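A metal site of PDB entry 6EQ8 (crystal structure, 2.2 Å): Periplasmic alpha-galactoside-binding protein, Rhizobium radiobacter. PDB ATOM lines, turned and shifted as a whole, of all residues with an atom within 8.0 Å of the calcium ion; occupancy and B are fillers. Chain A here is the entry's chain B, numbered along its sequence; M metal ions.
Of the 16 residues printed, 6 come within 4 Å of the calcium ion.
The nearest printed residue that does not touch the calcium ion is Thr 459 (4.3 Å).
ND2 of Asn 466 sits close to OG1 of Thr 459.
OD1 of Asp 458 sits close to N of Gly 461, 3.1 Å away.
The side-chain amide nitrogen (ND2) of Asn 466 sits at hydrogen-bond distance from the backbone carbonyl oxygen (O) of Gly 474.
OD2 of Asp 458 is in hydrogen-bond range of N of Gly 463 (2.9 Å).
The backbone carbonyl oxygen (O) of Lys 457 is in hydrogen-bond range of the backbone NH (N) of Asn 466, 3.0 Å away.
The calcium ion is bound by OD1 of Asp 460 (2.2 Å), O of Phe 464 (2.3 Å), OD1 of Asn 466 (2.3 Å), OD1 of Asn 476 (2.3 Å), OD1 of Asp 462 (2.3 Å) and OD1 of Asp 458 (2.5 Å).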
ATOM      1  N   LYS A 457     -20.126  19.313  22.505  1.00  0.00           N
ATOM      2  CA  LYS A 457     -18.869  18.674  22.885  1.00  0.00           C
ATOM      3  C   LYS A 457     -18.904  18.164  24.326  1.00  0.00           C
ATOM      4  O   LYS A 457     -19.614  18.719  25.162  1.00  0.00           O
ATOM      5  CB  LYS A 457     -17.634  19.558  22.610  1.00  0.00           C
ATOM      6  CG  LYS A 457     -17.496  20.828  23.435  1.00  0.00           C
ATOM      7  CD  LYS A 457     -16.138  21.489  23.169  1.00  0.00           C
ATOM      8  CE  LYS A 457     -15.682  22.404  24.289  1.00  0.00           C
ATOM      9  NZ  LYS A 457     -14.355  23.015  23.998  1.00  0.00           N
ATOM     10  N   ASP A 458     -18.151  17.081  24.599  1.00  0.00           N
ATOM     11  CA  ASP A 458     -18.038  16.496  25.938  1.00  0.00           C
ATOM     12  C   ASP A 458     -17.103  17.385  26.773  1.00  0.00           C
ATOM     13  O   ASP A 458     -15.885  17.376  26.577  1.00  0.00           O
ATOM     14  CB  ASP A 458     -17.555  15.045  25.866  1.00  0.00           C
ATOM     15  CG  ASP A 458     -17.351  14.364  27.195  1.00  0.00           C
ATOM     16  OD1 ASP A 458     -17.982  14.782  28.190  1.00  0.00           O
ATOM     17  OD2 ASP A 458     -16.561  13.399  27.251  1.00  0.00           O
ATOM     18  N   THR A 459     -17.701  18.188  27.685  1.00  0.00           N
ATOM     19  CA  THR A 459     -17.014  19.162  28.528  1.00  0.00           C
ATOM     20  C   THR A 459     -16.696  18.650  29.948  1.00  0.00           C
ATOM     21  O   THR A 459     -15.948  19.325  30.653  1.00  0.00           O
ATOM     22  CB  THR A 459     -17.789  20.502  28.578  1.00  0.00           C
ATOM     23  OG1 THR A 459     -19.071  20.305  29.166  1.00  0.00           O
ATOM     24  CG2 THR A 459     -17.912  21.162  27.213  1.00  0.00           C
ATOM     25  N   ASP A 460     -17.216  17.475  30.346  1.00  0.00           N
ATOM     26  CA  ASP A 460     -16.969  16.881  31.680  1.00  0.00           C
ATOM     27  C   ASP A 460     -16.215  15.518  31.635  1.00  0.00           C
ATOM     28  O   ASP A 460     -15.972  14.914  32.669  1.00  0.00           O
ATOM     29  CB  ASP A 460     -18.274  16.770  32.500  1.00  0.00           C
ATOM     30  CG  ASP A 460     -19.501  16.308  31.752  1.00  0.00           C
ATOM     31  OD1 ASP A 460     -19.361  15.422  30.875  1.00  0.00           O
ATOM     32  OD2 ASP A 460     -20.621  16.720  32.120  1.00  0.00           O
ATOM     33  N   GLY A 461     -15.884  15.043  30.435  1.00  0.00           N
ATOM     34  CA  GLY A 461     -15.145  13.794  30.229  1.00  0.00           C
ATOM     35  C   GLY A 461     -15.862  12.480  30.480  1.00  0.00           C
ATOM     36  O   GLY A 461     -15.201  11.480  30.759  1.00  0.00           O
ATOM     37  N   ASP A 462     -17.201  12.448  30.345  1.00  0.00           N
ATOM     38  CA  ASP A 462     -17.944  11.199  30.557  1.00  0.00           C
ATOM     39  C   ASP A 462     -18.290  10.452  29.241  1.00  0.00           C
ATOM     40  O   ASP A 462     -18.912   9.383  29.291  1.00  0.00           O
ATOM     41  CB  ASP A 462     -19.187  11.423  31.444  1.00  0.00           C
ATOM     42  CG  ASP A 462     -20.277  12.314  30.881  1.00  0.00           C
ATOM     43  OD1 ASP A 462     -20.056  12.912  29.782  1.00  0.00           O
ATOM     44  OD2 ASP A 462     -21.351  12.405  31.506  1.00  0.00           O
ATOM     45  N   GLY A 463     -17.867  10.995  28.094  1.00  0.00           N
ATOM     46  CA  GLY A 463     -18.129  10.408  26.783  1.00  0.00           C
ATOM     47  C   GLY A 463     -19.403  10.927  26.119  1.00  0.00           C
ATOM     48  O   GLY A 463     -19.586  10.753  24.909  1.00  0.00           O
ATOM     49  N   PHE A 464     -20.294  11.552  26.921  1.00  0.00           N
ATOM     50  CA  PHE A 464     -21.546  12.109  26.428  1.00  0.00           C
ATOM     51  C   PHE A 464     -21.377  13.590  26.081  1.00  0.00           C
ATOM     52  O   PHE A 464     -20.726  14.328  26.826  1.00  0.00           O
ATOM     53  CB  PHE A 464     -22.684  11.891  27.441  1.00  0.00           C
ATOM     54  CG  PHE A 464     -23.104  10.433  27.521  1.00  0.00           C
ATOM     55  CD1 PHE A 464     -23.938   9.884  26.559  1.00  0.00           C
ATOM     56  CD2 PHE A 464     -22.609   9.600  28.507  1.00  0.00           C
ATOM     57  CE1 PHE A 464     -24.296   8.529  26.616  1.00  0.00           C
ATOM     58  CE2 PHE A 464     -22.968   8.249  28.555  1.00  0.00           C
ATOM     59  CZ  PHE A 464     -23.822   7.730  27.616  1.00  0.00           C
ATOM     60  N   LEU A 465     -21.946  14.030  24.956  1.00  0.00           N
ATOM     61  CA  LEU A 465     -21.890  15.426  24.537  1.00  0.00           C
ATOM     62  C   LEU A 465     -22.767  16.311  25.427  1.00  0.00           C
ATOM     63  O   LEU A 465     -23.855  15.927  25.870  1.00  0.00           O
ATOM     64  CB  LEU A 465     -22.283  15.600  23.062  1.00  0.00           C
ATOM     65  CG  LEU A 465     -21.484  14.809  22.010  1.00  0.00           C
ATOM     66  CD1 LEU A 465     -22.142  14.894  20.666  1.00  0.00           C
ATOM     67  CD2 LEU A 465     -20.058  15.246  21.937  1.00  0.00           C
ATOM     68  N   ASN A 466     -22.252  17.494  25.690  1.00  0.00           N
ATOM     69  CA  ASN A 466     -22.895  18.503  26.505  1.00  0.00           C
ATOM     70  C   ASN A 466     -23.346  19.634  25.627  1.00  0.00           C
ATOM     71  O   ASN A 466     -22.690  19.950  24.627  1.00  0.00           O
ATOM     72  CB  ASN A 466     -21.887  19.090  27.517  1.00  0.00           C
ATOM     73  CG  ASN A 466     -21.363  18.108  28.503  1.00  0.00           C
ATOM     74  OD1 ASN A 466     -20.585  17.191  28.174  1.00  0.00           O
ATOM     75  ND2 ASN A 466     -21.766  18.296  29.738  1.00  0.00           N
ATOM     76  N   PHE A 467     -24.435  20.300  26.037  1.00  0.00           N
ATOM     77  CA  PHE A 467     -24.957  21.506  25.403  1.00  0.00           C
ATOM     78  C   PHE A 467     -23.940  22.631  25.644  1.00  0.00           C
ATOM     79  O   PHE A 467     -23.134  22.516  26.583  1.00  0.00           O
ATOM     80  CB  PHE A 467     -26.276  21.917  26.096  1.00  0.00           C
ATOM     81  CG  PHE A 467     -27.492  21.083  25.782  1.00  0.00           C
ATOM     82  CD1 PHE A 467     -28.126  21.189  24.549  1.00  0.00           C
ATOM     83  CD2 PHE A 467     -28.030  20.224  26.724  1.00  0.00           C
ATOM     84  CE1 PHE A 467     -29.268  20.446  24.269  1.00  0.00           C
ATOM     85  CE2 PHE A 467     -29.146  19.442  26.429  1.00  0.00           C
ATOM     86  CZ  PHE A 467     -29.778  19.588  25.209  1.00  0.00           C
ATOM     87  N   GLY A 474     -24.883  23.987  30.348  1.00  0.00           N
ATOM     88  CA  GLY A 474     -23.864  23.158  29.698  1.00  0.00           C
ATOM     89  C   GLY A 474     -23.944  21.689  30.094  1.00  0.00           C
ATOM     90  O   GLY A 474     -22.947  20.964  30.087  1.00  0.00           O
ATOM     91  N   ARG A 475     -25.153  21.249  30.444  1.00  0.00           N
ATOM     92  CA  ARG A 475     -25.442  19.889  30.886  1.00  0.00           C
ATOM     93  C   ARG A 475     -25.421  18.909  29.701  1.00  0.00           C
ATOM     94  O   ARG A 475     -25.496  19.332  28.547  1.00  0.00           O
ATOM     95  CB  ARG A 475     -26.746  19.878  31.719  1.00  0.00           C
ATOM     96  CG  ARG A 475     -28.011  19.190  31.268  1.00  0.00           C
ATOM     97  CD  ARG A 475     -28.880  18.982  32.516  1.00  0.00           C
ATOM     98  NE  ARG A 475     -29.476  20.235  32.986  1.00  0.00           N
ATOM     99  CZ  ARG A 475     -30.775  20.426  33.157  1.00  0.00           C
ATOM    100  NH1 ARG A 475     -31.635  19.442  32.929  1.00  0.00           N
ATOM    101  NH2 ARG A 475     -31.232  21.599  33.587  1.00  0.00           N
ATOM    102  N   ASN A 476     -25.204  17.620  30.005  1.00  0.00           N
ATOM    103  CA  ASN A 476     -25.196  16.552  28.992  1.00  0.00           C
ATOM    104  C   ASN A 476     -26.555  16.500  28.300  1.00  0.00           C
ATOM    105  O   ASN A 476     -27.593  16.652  28.943  1.00  0.00           O
ATOM    106  CB  ASN A 476     -24.957  15.174  29.624  1.00  0.00           C
ATOM    107  CG  ASN A 476     -23.531  14.865  29.922  1.00  0.00           C
ATOM    108  OD1 ASN A 476     -22.660  14.984  29.089  1.00  0.00           O
ATOM    109  ND2 ASN A 476     -23.289  14.370  31.120  1.00  0.00           N
ATOM    110  N   VAL A 477     -26.527  16.272  26.989  1.00  0.00           N
ATOM    111  CA  VAL A 477     -27.727  16.126  26.166  1.00  0.00           C
ATOM    112  C   VAL A 477     -28.424  14.813  26.565  1.00  0.00           C
ATOM    113  O   VAL A 477     -27.782  13.764  26.637  1.00  0.00           O
ATOM    114  CB  VAL A 477     -27.364  16.214  24.647  1.00  0.00           C
ATOM    115  CG1 VAL A 477     -28.597  16.027  23.771  1.00  0.00           C
ATOM    116  CG2 VAL A 477     -26.674  17.548  24.320  1.00  0.00           C
ATOM    117  N   GLY A 505     -22.419   9.887  21.133  1.00  0.00           N
ATOM    118  CA  GLY A 505     -22.230  10.755  22.282  1.00  0.00           C
ATOM    119  C   GLY A 505     -23.547  11.290  22.827  1.00  0.00           C
ATOM    120  O   GLY A 505     -23.548  12.246  23.599  1.00  0.00           O
HETATM  121 CA    CA M   1     -20.389  15.054  28.932  1.00  0.00          CA
